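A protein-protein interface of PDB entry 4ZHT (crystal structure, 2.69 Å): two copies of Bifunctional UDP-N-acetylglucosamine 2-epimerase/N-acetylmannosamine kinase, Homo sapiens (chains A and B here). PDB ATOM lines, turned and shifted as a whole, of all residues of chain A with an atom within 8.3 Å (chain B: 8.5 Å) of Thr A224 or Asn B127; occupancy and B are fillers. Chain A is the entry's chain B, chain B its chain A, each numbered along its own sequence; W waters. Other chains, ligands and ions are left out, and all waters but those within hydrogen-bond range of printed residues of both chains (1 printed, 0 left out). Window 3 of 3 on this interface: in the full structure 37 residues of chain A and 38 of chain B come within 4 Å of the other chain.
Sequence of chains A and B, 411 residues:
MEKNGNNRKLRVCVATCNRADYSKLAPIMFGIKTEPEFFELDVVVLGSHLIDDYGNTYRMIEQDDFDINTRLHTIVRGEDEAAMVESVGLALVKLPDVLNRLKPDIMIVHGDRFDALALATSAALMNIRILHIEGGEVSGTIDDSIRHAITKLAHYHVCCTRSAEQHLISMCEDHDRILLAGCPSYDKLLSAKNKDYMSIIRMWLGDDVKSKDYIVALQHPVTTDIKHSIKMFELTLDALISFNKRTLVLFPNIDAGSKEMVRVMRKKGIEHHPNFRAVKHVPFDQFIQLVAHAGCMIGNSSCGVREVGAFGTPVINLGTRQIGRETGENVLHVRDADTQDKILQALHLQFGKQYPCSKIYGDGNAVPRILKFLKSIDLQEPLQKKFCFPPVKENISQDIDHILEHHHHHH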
ATOM      1  N   GLU A  81      12.442   9.115   2.152  1.00  0.00           N
ATOM      2  CA  GLU A  81      13.770   9.329   1.665  1.00  0.00           C
ATOM      3  C   GLU A  81      14.796   8.518   2.439  1.00  0.00           C
ATOM      4  O   GLU A  81      15.687   7.929   1.815  1.00  0.00           O
ATOM      5  CB  GLU A  81      14.105  10.818   1.720  1.00  0.00           C
ATOM      6  CG  GLU A  81      13.222  11.644   0.812  1.00  0.00           C
ATOM      7  CD  GLU A  81      12.858  13.009   1.331  1.00  0.00           C
ATOM      8  OE1 GLU A  81      12.718  13.764   0.391  1.00  0.00           O
ATOM      9  OE2 GLU A  81      12.723  13.366   2.543  1.00  0.00           O
ATOM     10  N   ALA A  82      14.706   8.498   3.776  1.00  0.00           N
ATOM     11  CA  ALA A  82      15.626   7.668   4.552  1.00  0.00           C
ATOM     12  C   ALA A  82      15.588   6.218   4.062  1.00  0.00           C
ATOM     13  O   ALA A  82      16.630   5.623   3.873  1.00  0.00           O
ATOM     14  CB  ALA A  82      15.298   7.723   6.014  1.00  0.00           C
ATOM     15  N   VAL A  85      17.360   5.554   0.795  1.00  0.00           N
ATOM     16  CA  VAL A  85      18.803   5.448   0.940  1.00  0.00           C
ATOM     17  C   VAL A  85      19.225   4.110   1.544  1.00  0.00           C
ATOM     18  O   VAL A  85      20.215   3.519   1.103  1.00  0.00           O
ATOM     19  CB  VAL A  85      19.389   6.622   1.729  1.00  0.00           C
ATOM     20  CG1 VAL A  85      20.873   6.436   2.020  1.00  0.00           C
ATOM     21  CG2 VAL A  85      19.202   7.891   0.920  1.00  0.00           C
ATOM     22  N   GLY A 140      14.662  16.742 -15.121  1.00  0.00           N
ATOM     23  CA  GLY A 140      14.441  17.797 -14.135  1.00  0.00           C
ATOM     24  C   GLY A 140      13.986  17.420 -12.731  1.00  0.00           C
ATOM     25  O   GLY A 140      13.169  18.128 -12.141  1.00  0.00           O
ATOM     26  N   THR A 141      14.480  16.307 -12.205  1.00  0.00           N
ATOM     27  CA  THR A 141      14.368  16.021 -10.770  1.00  0.00           C
ATOM     28  C   THR A 141      15.724  15.575 -10.267  1.00  0.00           C
ATOM     29  O   THR A 141      16.706  15.619 -11.003  1.00  0.00           O
ATOM     30  CB  THR A 141      13.288  14.947 -10.446  1.00  0.00           C
ATOM     31  OG1 THR A 141      13.611  13.695 -11.079  1.00  0.00           O
ATOM     32  CG2 THR A 141      11.920  15.405 -10.917  1.00  0.00           C
ATOM     33  N   ILE A 142      15.780  15.139  -9.014  1.00  0.00           N
ATOM     34  CA  ILE A 142      16.945  14.427  -8.493  1.00  0.00           C
ATOM     35  C   ILE A 142      17.449  13.314  -9.452  1.00  0.00           C
ATOM     36  O   ILE A 142      18.635  12.998  -9.459  1.00  0.00           O
ATOM     37  CB  ILE A 142      16.641  13.887  -7.078  1.00  0.00           C
ATOM     38  CG1 ILE A 142      17.882  13.290  -6.396  1.00  0.00           C
ATOM     39  CG2 ILE A 142      15.525  12.841  -7.106  1.00  0.00           C
ATOM     40  CD1 ILE A 142      19.031  14.250  -6.229  1.00  0.00           C
ATOM     41  N   ASP A 143      16.557  12.753 -10.269  1.00  0.00           N
ATOM     42  CA  ASP A 143      16.909  11.669 -11.188  1.00  0.00           C
ATOM     43  C   ASP A 143      17.995  12.053 -12.206  1.00  0.00           C
ATOM     44  O   ASP A 143      18.817  11.222 -12.573  1.00  0.00           O
ATOM     45  CB  ASP A 143      15.655  11.105 -11.900  1.00  0.00           C
ATOM     46  CG  ASP A 143      14.529  10.669 -10.918  1.00  0.00           C
ATOM     47  OD1 ASP A 143      14.795  10.411  -9.710  1.00  0.00           O
ATOM     48  OD2 ASP A 143      13.355  10.623 -11.366  1.00  0.00           O
ATOM     49  N   PRO A 221       5.118  10.740  -7.109  1.00  0.00           N
ATOM     50  CA  PRO A 221       5.584  11.820  -6.238  1.00  0.00           C
ATOM     51  C   PRO A 221       6.993  12.251  -6.639  1.00  0.00           C
ATOM     52  O   PRO A 221       7.749  11.452  -7.196  1.00  0.00           O
ATOM     53  CB  PRO A 221       5.589  11.172  -4.869  1.00  0.00           C
ATOM     54  CG  PRO A 221       5.895   9.740  -5.160  1.00  0.00           C
ATOM     55  CD  PRO A 221       5.180   9.432  -6.438  1.00  0.00           C
ATOM     56  N   VAL A 222       7.292  13.537  -6.451  1.00  0.00           N
ATOM     57  CA  VAL A 222       8.641  14.070  -6.626  1.00  0.00           C
ATOM     58  C   VAL A 222       9.179  14.149  -5.215  1.00  0.00           C
ATOM     59  O   VAL A 222       8.567  14.775  -4.353  1.00  0.00           O
ATOM     60  CB  VAL A 222       8.634  15.463  -7.276  1.00  0.00           C
ATOM     61  CG1 VAL A 222      10.052  16.016  -7.423  1.00  0.00           C
ATOM     62  CG2 VAL A 222       7.965  15.407  -8.639  1.00  0.00           C
ATOM     63  N   THR A 223      10.339  13.535  -5.002  1.00  0.00           N
ATOM     64  CA  THR A 223      10.859  13.271  -3.648  1.00  0.00           C
ATOM     65  C   THR A 223      11.308  14.569  -2.948  1.00  0.00           C
ATOM     66  O   THR A 223      11.259  14.685  -1.714  1.00  0.00           O
ATOM     67  CB  THR A 223      12.042  12.269  -3.685  1.00  0.00           C
ATOM     68  OG1 THR A 223      13.177  12.872  -4.344  1.00  0.00           O
ATOM     69  CG2 THR A 223      11.647  10.973  -4.407  1.00  0.00           C
ATOM     70  N   THR A 224      11.721  15.533  -3.770  1.00  0.00           N
ATOM     71  CA  THR A 224      12.214  16.825  -3.326  1.00  0.00           C
ATOM     72  C   THR A 224      11.119  17.669  -2.686  1.00  0.00           C
ATOM     73  O   THR A 224      11.422  18.470  -1.817  1.00  0.00           O
ATOM     74  CB  THR A 224      12.861  17.624  -4.498  1.00  0.00           C
ATOM     75  OG1 THR A 224      11.841  18.188  -5.326  1.00  0.00           O
ATOM     76  CG2 THR A 224      13.768  16.749  -5.397  1.00  0.00           C
ATOM     77  N   ASP A 225       9.867  17.513  -3.133  1.00  0.00           N
ATOM     78  CA  ASP A 225       8.730  18.324  -2.644  1.00  0.00           C
ATOM     79  C   ASP A 225       7.460  17.450  -2.507  1.00  0.00           C
ATOM     80  O   ASP A 225       6.524  17.542  -3.311  1.00  0.00           O
ATOM     81  CB  ASP A 225       8.476  19.534  -3.582  1.00  0.00           C
ATOM     82  CG  ASP A 225       7.654  20.662  -2.923  1.00  0.00           C
ATOM     83  OD1 ASP A 225       6.969  20.411  -1.912  1.00  0.00           O
ATOM     84  OD2 ASP A 225       7.666  21.816  -3.427  1.00  0.00           O
ATOM     85  N   ILE A 226       7.437  16.606  -1.478  1.00  0.00           N
ATOM     86  CA  ILE A 226       6.283  15.729  -1.238  1.00  0.00           C
ATOM     87  C   ILE A 226       4.996  16.503  -0.968  1.00  0.00           C
ATOM     88  O   ILE A 226       3.976  16.185  -1.549  1.00  0.00           O
ATOM     89  CB  ILE A 226       6.571  14.612  -0.177  1.00  0.00           C
ATOM     90  CG1 ILE A 226       7.505  13.544  -0.796  1.00  0.00           C
ATOM     91  CG2 ILE A 226       5.285  13.945   0.323  1.00  0.00           C
ATOM     92  CD1 ILE A 226       8.081  12.492   0.140  1.00  0.00           C
ATOM     93  N   LYS A 227       5.049  17.560  -0.174  1.00  0.00           N
ATOM     94  CA  LYS A 227       3.824  18.299   0.142  1.00  0.00           C
ATOM     95  C   LYS A 227       3.143  18.889  -1.095  1.00  0.00           C
ATOM     96  O   LYS A 227       1.902  18.924  -1.183  1.00  0.00           O
ATOM     97  CB  LYS A 227       4.138  19.387   1.193  1.00  0.00           C
ATOM     98  CG  LYS A 227       4.658  18.801   2.518  1.00  0.00           C
ATOM     99  CD  LYS A 227       4.125  19.478   3.796  1.00  0.00           C
ATOM    100  CE  LYS A 227       3.791  18.472   4.908  1.00  0.00           C
ATOM    101  NZ  LYS A 227       2.519  18.814   5.609  1.00  0.00           N
ATOM    102  N   HIS A 228       3.957  19.306  -2.061  1.00  0.00           N
ATOM    103  CA  HIS A 228       3.451  19.796  -3.342  1.00  0.00           C
ATOM    104  C   HIS A 228       2.941  18.646  -4.227  1.00  0.00           C
ATOM    105  O   HIS A 228       1.893  18.782  -4.878  1.00  0.00           O
ATOM    106  CB  HIS A 228       4.513  20.647  -4.067  1.00  0.00           C
ATOM    107  CG  HIS A 228       3.996  21.379  -5.274  1.00  0.00           C
ATOM    108  ND1 HIS A 228       2.740  21.954  -5.344  1.00  0.00           N
ATOM    109  CD2 HIS A 228       4.580  21.610  -6.472  1.00  0.00           C
ATOM    110  CE1 HIS A 228       2.572  22.499  -6.536  1.00  0.00           C
ATOM    111  NE2 HIS A 228       3.675  22.306  -7.239  1.00  0.00           N
ATOM    112  N   SER A 229       3.655  17.521  -4.238  1.00  0.00           N
ATOM    113  CA  SER A 229       3.177  16.316  -4.927  1.00  0.00           C
ATOM    114  C   SER A 229       1.785  15.880  -4.459  1.00  0.00           C
ATOM    115  O   SER A 229       0.953  15.485  -5.286  1.00  0.00           O
ATOM    116  CB  SER A 229       4.152  15.168  -4.739  1.00  0.00           C
ATOM    117  OG  SER A 229       5.369  15.431  -5.389  1.00  0.00           O
ATOM    118  N   ILE A 254       7.101   5.844  -7.467  1.00  0.00           N
ATOM    119  CA  ILE A 254       8.325   6.289  -6.824  1.00  0.00           C
ATOM    120  C   ILE A 254       8.054   6.076  -5.339  1.00  0.00           C
ATOM    121  O   ILE A 254       7.012   6.477  -4.826  1.00  0.00           O
ATOM    122  CB  ILE A 254       8.616   7.771  -7.087  1.00  0.00           C
ATOM    123  CG1 ILE A 254       8.889   8.023  -8.580  1.00  0.00           C
ATOM    124  CG2 ILE A 254       9.777   8.265  -6.233  1.00  0.00           C
ATOM    125  CD1 ILE A 254      10.203   7.460  -9.105  1.00  0.00           C
ATOM    126  N   ALA A 256       9.410   7.154  -2.264  1.00  0.00           N
ATOM    127  CA  ALA A 256       9.358   8.188  -1.241  1.00  0.00           C
ATOM    128  C   ALA A 256       8.146   9.043  -1.474  1.00  0.00           C
ATOM    129  O   ALA A 256       8.002   9.639  -2.525  1.00  0.00           O
ATOM    130  CB  ALA A 256      10.601   9.031  -1.271  1.00  0.00           C
ATOM    131  N   THR A 320       6.900  19.233 -12.358  1.00  0.00           N
ATOM    132  CA  THR A 320       8.313  19.469 -12.652  1.00  0.00           C
ATOM    133  C   THR A 320       9.031  18.241 -13.176  1.00  0.00           C
ATOM    134  O   THR A 320      10.076  18.362 -13.809  1.00  0.00           O
ATOM    135  CB  THR A 320       9.069  19.912 -11.393  1.00  0.00           C
ATOM    136  OG1 THR A 320       8.866  18.933 -10.357  1.00  0.00           O
ATOM    137  CG2 THR A 320       8.584  21.277 -10.949  1.00  0.00           C
ATOM    138  N   PRO B 104      21.214  18.577   9.165  1.00  0.00           N
ATOM    139  CA  PRO B 104      22.168  19.518   8.580  1.00  0.00           C
ATOM    140  C   PRO B 104      21.624  20.299   7.382  1.00  0.00           C
ATOM    141  O   PRO B 104      20.834  19.777   6.620  1.00  0.00           O
ATOM    142  CB  PRO B 104      23.300  18.616   8.108  1.00  0.00           C
ATOM    143  CG  PRO B 104      22.620  17.370   7.735  1.00  0.00           C
ATOM    144  CD  PRO B 104      21.526  17.201   8.755  1.00  0.00           C
ATOM    145  N   ASP B 105      22.066  21.545   7.228  1.00  0.00           N
ATOM    146  CA  ASP B 105      21.745  22.335   6.052  1.00  0.00           C
ATOM    147  C   ASP B 105      22.655  21.977   4.905  1.00  0.00           C
ATOM    148  O   ASP B 105      22.246  22.080   3.745  1.00  0.00           O
ATOM    149  CB  ASP B 105      21.868  23.820   6.350  1.00  0.00           C
ATOM    150  CG  ASP B 105      20.847  24.270   7.337  1.00  0.00           C
ATOM    151  OD1 ASP B 105      19.633  24.038   7.122  1.00  0.00           O
ATOM    152  OD2 ASP B 105      21.248  24.877   8.362  1.00  0.00           O
ATOM    153  N   ILE B 106      23.893  21.610   5.227  1.00  0.00           N
ATOM    154  CA  ILE B 106      24.851  21.219   4.221  1.00  0.00           C
ATOM    155  C   ILE B 106      25.807  20.209   4.801  1.00  0.00           C
ATOM    156  O   ILE B 106      26.138  20.256   5.987  1.00  0.00           O
ATOM    157  CB  ILE B 106      25.621  22.453   3.644  1.00  0.00           C
ATOM    158  CG1 ILE B 106      26.515  22.047   2.474  1.00  0.00           C
ATOM    159  CG2 ILE B 106      26.476  23.155   4.695  1.00  0.00           C
ATOM    160  CD1 ILE B 106      26.778  23.178   1.511  1.00  0.00           C
ATOM    161  N   ALA B 120      27.921  11.203  -0.254  1.00  0.00           N
ATOM    162  CA  ALA B 120      27.275  11.994  -1.274  1.00  0.00           C
ATOM    163  C   ALA B 120      25.918  11.424  -1.636  1.00  0.00           C
ATOM    164  O   ALA B 120      24.944  12.159  -1.793  1.00  0.00           O
ATOM    165  CB  ALA B 120      28.161  12.094  -2.510  1.00  0.00           C
ATOM    166  N   THR B 121      25.844  10.108  -1.747  1.00  0.00           N
ATOM    167  CA  THR B 121      24.616   9.443  -2.161  1.00  0.00           C
ATOM    168  C   THR B 121      23.526   9.707  -1.166  1.00  0.00           C
ATOM    169  O   THR B 121      22.397  10.072  -1.537  1.00  0.00           O
ATOM    170  CB  THR B 121      24.841   7.921  -2.344  1.00  0.00           C
ATOM    171  OG1 THR B 121      25.801   7.710  -3.387  1.00  0.00           O
ATOM    172  CG2 THR B 121      23.555   7.195  -2.732  1.00  0.00           C
ATOM    173  N   SER B 122      23.867   9.515   0.102  1.00  0.00           N
ATOM    174  CA  SER B 122      22.879   9.624   1.171  1.00  0.00           C
ATOM    175  C   SER B 122      22.371  11.052   1.287  1.00  0.00           C
ATOM    176  O   SER B 122      21.167  11.279   1.332  1.00  0.00           O
ATOM    177  CB  SER B 122      23.453   9.094   2.480  1.00  0.00           C
ATOM    178  OG  SER B 122      24.401   9.976   3.015  1.00  0.00           O
ATOM    179  N   ALA B 123      23.281  12.027   1.227  1.00  0.00           N
ATOM    180  CA  ALA B 123      22.880  13.449   1.247  1.00  0.00           C
ATOM    181  C   ALA B 123      21.997  13.858   0.067  1.00  0.00           C
ATOM    182  O   ALA B 123      20.952  14.478   0.268  1.00  0.00           O
ATOM    183  CB  ALA B 123      24.094  14.326   1.271  1.00  0.00           C
ATOM    184  N   ALA B 124      22.421  13.477  -1.148  1.00  0.00           N
ATOM    185  CA  ALA B 124      21.701  13.819  -2.368  1.00  0.00           C
ATOM    186  C   ALA B 124      20.310  13.255  -2.401  1.00  0.00           C
ATOM    187  O   ALA B 124      19.360  13.950  -2.717  1.00  0.00           O
ATOM    188  CB  ALA B 124      22.448  13.325  -3.567  1.00  0.00           C
ATOM    189  N   LEU B 125      20.161  11.991  -2.020  1.00  0.00           N
ATOM    190  CA  LEU B 125      18.829  11.360  -2.043  1.00  0.00           C
ATOM    191  C   LEU B 125      17.913  11.832  -0.920  1.00  0.00           C
ATOM    192  O   LEU B 125      16.710  11.697  -1.022  1.00  0.00           O
ATOM    193  CB  LEU B 125      18.961   9.842  -2.031  1.00  0.00           C
ATOM    194  CG  LEU B 125      19.473   9.227  -3.336  1.00  0.00           C
ATOM    195  CD1 LEU B 125      19.813   7.770  -3.089  1.00  0.00           C
ATOM    196  CD2 LEU B 125      18.424   9.314  -4.438  1.00  0.00           C
ATOM    197  N   MET B 126      18.485  12.411   0.132  1.00  0.00           N
ATOM    198  CA  MET B 126      17.689  13.014   1.223  1.00  0.00           C
ATOM    199  C   MET B 126      17.550  14.513   1.113  1.00  0.00           C
ATOM    200  O   MET B 126      17.101  15.158   2.060  1.00  0.00           O
ATOM    201  CB  MET B 126      18.331  12.639   2.547  1.00  0.00           C
ATOM    202  CG  MET B 126      18.119  11.160   2.725  1.00  0.00           C
ATOM    203  SD  MET B 126      18.728  10.775   4.543  1.00  0.00           S
ATOM    204  CE  MET B 126      20.544  10.297   4.038  1.00  0.00           C
ATOM    205  N   ASN B 127      17.883  15.088  -0.051  1.00  0.00           N
ATOM    206  CA  ASN B 127      17.795  16.535  -0.230  1.00  0.00           C
ATOM    207  C   ASN B 127      18.603  17.375   0.745  1.00  0.00           C
ATOM    208  O   ASN B 127      18.189  18.452   1.105  1.00  0.00           O
ATOM    209  CB  ASN B 127      16.325  16.982  -0.231  1.00  0.00           C
ATOM    210  CG  ASN B 127      15.908  17.391  -1.602  1.00  0.00           C
ATOM    211  OD1 ASN B 127      16.232  18.486  -2.067  1.00  0.00           O
ATOM    212  ND2 ASN B 127      15.338  16.430  -2.332  1.00  0.00           N
ATOM    213  N   ILE B 128      19.757  16.873   1.154  1.00  0.00           N
ATOM    214  CA  ILE B 128      20.689  17.647   1.940  1.00  0.00           C
ATOM    215  C   ILE B 128      21.751  18.164   0.962  1.00  0.00           C
ATOM    216  O   ILE B 128      22.295  17.395   0.171  1.00  0.00           O
ATOM    217  CB  ILE B 128      21.321  16.802   3.039  1.00  0.00           C
ATOM    218  CG1 ILE B 128      20.253  16.342   4.020  1.00  0.00           C
ATOM    219  CG2 ILE B 128      22.376  17.590   3.794  1.00  0.00           C
ATOM    220  CD1 ILE B 128      20.704  15.180   4.902  1.00  0.00           C
ATOM    221  N   ARG B 129      22.043  19.459   1.029  1.00  0.00           N
ATOM    222  CA  ARG B 129      23.078  20.070   0.196  1.00  0.00           C
ATOM    223  C   ARG B 129      24.464  19.514   0.473  1.00  0.00           C
ATOM    224  O   ARG B 129      24.774  19.185   1.618  1.00  0.00           O
ATOM    225  CB  ARG B 129      23.147  21.560   0.465  1.00  0.00           C
ATOM    226  CG  ARG B 129      21.911  22.338   0.086  1.00  0.00           C
ATOM    227  CD  ARG B 129      22.123  23.772   0.495  1.00  0.00           C
ATOM    228  NE  ARG B 129      21.126  24.623  -0.129  1.00  0.00           N
ATOM    229  CZ  ARG B 129      19.878  24.760   0.303  1.00  0.00           C
ATOM    230  NH1 ARG B 129      19.446  24.093   1.392  1.00  0.00           N
ATOM    231  NH2 ARG B 129      19.052  25.582  -0.352  1.00  0.00           N
ATOM    232  N   ILE B 130      25.294  19.472  -0.568  1.00  0.00           N
ATOM    233  CA  ILE B 130      26.619  18.863  -0.525  1.00  0.00           C
ATOM    234  C   ILE B 130      27.660  19.850  -1.043  1.00  0.00           C
ATOM    235  O   ILE B 130      27.514  20.424  -2.138  1.00  0.00           O
ATOM    236  CB  ILE B 130      26.742  17.617  -1.420  1.00  0.00           C
ATOM    237  CG1 ILE B 130      25.785  16.519  -0.981  1.00  0.00           C
ATOM    238  CG2 ILE B 130      28.179  17.056  -1.393  1.00  0.00           C
ATOM    239  CD1 ILE B 130      25.467  15.540  -2.102  1.00  0.00           C
ATOM    240  N   HIS B 155      26.072  19.517  -5.036  1.00  0.00           N
ATOM    241  CA  HIS B 155      25.410  20.748  -5.388  1.00  0.00           C
ATOM    242  C   HIS B 155      26.398  21.913  -5.461  1.00  0.00           C
ATOM    243  O   HIS B 155      26.163  22.852  -6.198  1.00  0.00           O
ATOM    244  CB  HIS B 155      24.338  21.050  -4.340  1.00  0.00           C
ATOM    245  CG  HIS B 155      23.396  19.914  -4.110  1.00  0.00           C
ATOM    246  ND1 HIS B 155      23.667  18.885  -3.234  1.00  0.00           N
ATOM    247  CD2 HIS B 155      22.186  19.647  -4.644  1.00  0.00           C
ATOM    248  CE1 HIS B 155      22.665  18.031  -3.245  1.00  0.00           C
ATOM    249  NE2 HIS B 155      21.748  18.477  -4.084  1.00  0.00           N
ATOM    250  N   GLU B 381      16.138  26.437  -2.627  1.00  0.00           N
ATOM    251  CA  GLU B 381      15.760  25.604  -3.787  1.00  0.00           C
ATOM    252  C   GLU B 381      15.552  24.136  -3.309  1.00  0.00           C
ATOM    253  O   GLU B 381      14.410  23.858  -2.928  1.00  0.00           O
ATOM    254  CB  GLU B 381      16.640  25.823  -5.021  1.00  0.00           C
ATOM    255  CG  GLU B 381      16.077  25.206  -6.294  1.00  0.00           C
ATOM    256  CD  GLU B 381      16.958  25.444  -7.523  1.00  0.00           C
ATOM    257  OE1 GLU B 381      17.843  26.332  -7.497  1.00  0.00           O
ATOM    258  OE2 GLU B 381      16.753  24.749  -8.541  1.00  0.00           O
ATOM    259  N   PRO B 382      16.517  23.180  -3.291  1.00  0.00           N
ATOM    260  CA  PRO B 382      17.713  23.046  -4.128  1.00  0.00           C
ATOM    261  C   PRO B 382      17.405  22.122  -5.304  1.00  0.00           C
ATOM    262  O   PRO B 382      16.503  21.287  -5.219  1.00  0.00           O
ATOM    263  CB  PRO B 382      18.710  22.347  -3.192  1.00  0.00           C
ATOM    264  CG  PRO B 382      17.865  21.484  -2.314  1.00  0.00           C
ATOM    265  CD  PRO B 382      16.487  22.127  -2.247  1.00  0.00           C
ATOM    266  N   LEU B 383      18.136  22.285  -6.388  1.00  0.00           N
ATOM    267  CA  LEU B 383      18.124  21.319  -7.479  1.00  0.00           C
ATOM    268  C   LEU B 383      19.307  21.680  -8.328  1.00  0.00           C
ATOM    269  O   LEU B 383      19.537  22.854  -8.630  1.00  0.00           O
ATOM    270  CB  LEU B 383      16.835  21.361  -8.322  1.00  0.00           C
ATOM    271  CG  LEU B 383      16.650  20.306  -9.435  1.00  0.00           C
ATOM    272  CD1 LEU B 383      16.481  18.905  -8.871  1.00  0.00           C
ATOM    273  CD2 LEU B 383      15.446  20.645 -10.296  1.00  0.00           C
ATOM    274  N   GLN B 384      20.065  20.668  -8.706  1.00  0.00           N
ATOM    275  CA  GLN B 384      21.274  20.870  -9.471  1.00  0.00           C
ATOM    276  C   GLN B 384      20.883  21.282 -10.908  1.00  0.00           C
ATOM    277  O   GLN B 384      19.851  20.862 -11.431  1.00  0.00           O
ATOM    278  CB  GLN B 384      22.157  19.602  -9.412  1.00  0.00           C
ATOM    279  CG  GLN B 384      23.637  19.849  -9.699  1.00  0.00           C
ATOM    280  CD  GLN B 384      24.548  18.735  -9.246  1.00  0.00           C
ATOM    281  OE1 GLN B 384      24.197  18.000  -8.346  1.00  0.00           O
ATOM    282  NE2 GLN B 384      25.736  18.626  -9.843  1.00  0.00           N
HETATM  283  O   HOH W   1      14.892  12.755  -2.299  1.00  0.00           O
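Water W1 lies within hydrogen-bond range of the backbone carbonyl oxygen of Leu B125 (2.5 Å) and the side-chain hydroxyl of Thr A223 (2.7 Å).
No position is printed for both chains. Of the 9 pairs that touch across the chains among the printed residues, none has its exchanged pair printed and touching as well.
The side-chain carboxylate (OE1) of Glu A81 sits close to the backbone carbonyl oxygen (O) of Thr A223, at 2.7 Å. The side-chain carboxylate (OD2) of Asp A143 lies within hydrogen-bond range of the side-chain hydroxyl (OG1) of Thr A141, 3.1 Å away.
CB of Glu A81 touches O of Leu B125, at 3.9 Å. CB of Ser B122 touches CG1 of Val A85 (3.7 Å). Val A85 touches Leu B125 (CG2 to CB, 3.5 Å). Met B126 touches Val A85 (CG to CG2, 3.9 Å). O of Gly A140 touches CD2 of Leu B383, at 3.9 Å. Thr A141 touches Leu B383 (C to CD1, 3.7 Å). Ala B124 touches Ile A142 (O to CD1, 3.5 Å). Leu B383 touches Ile A142 (CD1 to N, 3.8 Å). Asn B127 touches Thr A224 (ND2 to CA, 3.3 Å).
Printed residues of chain B that touch a printed residue of chain A: Ser B122, Ala B124, Leu B125, Met B126, Asn B127 and Leu B383. Hydrophobic or aromatic side chains of chain B within 4 Å of the printed part of chain A: Leu B125, Met B126 and Leu B383. Hydrophobic or aromatic side chains of chain A that line the printed part of chain B: Val A85 and Ile A142. Among the printed residues, 9 pairs touch across the chains. Among the printed residues, no Asp or Glu carboxylate lies within 4 Å of a Lys or Arg side-chain nitrogen of the other chain.
Printed residues of chain B within 4 Å of Val A85: Ser B122, Leu B125 and Met B126. Of the printed residues of chain B, Gly A140 touches Leu B383 (3.9 Å). Of the printed residues of chain B, Ile A142 touches Ala B124 (3.5 Å) and Leu B383 (3.8 Å). Thr A224 touches one residue of chain B. Of the printed residues of chain A, Ser B122 touches Val A85 (3.7 Å). Asn B127 touches just one residue of chain A: Thr A224. The nearest residue of chain B that does not touch Thr A224 is Leu B383 (4.9 Å).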
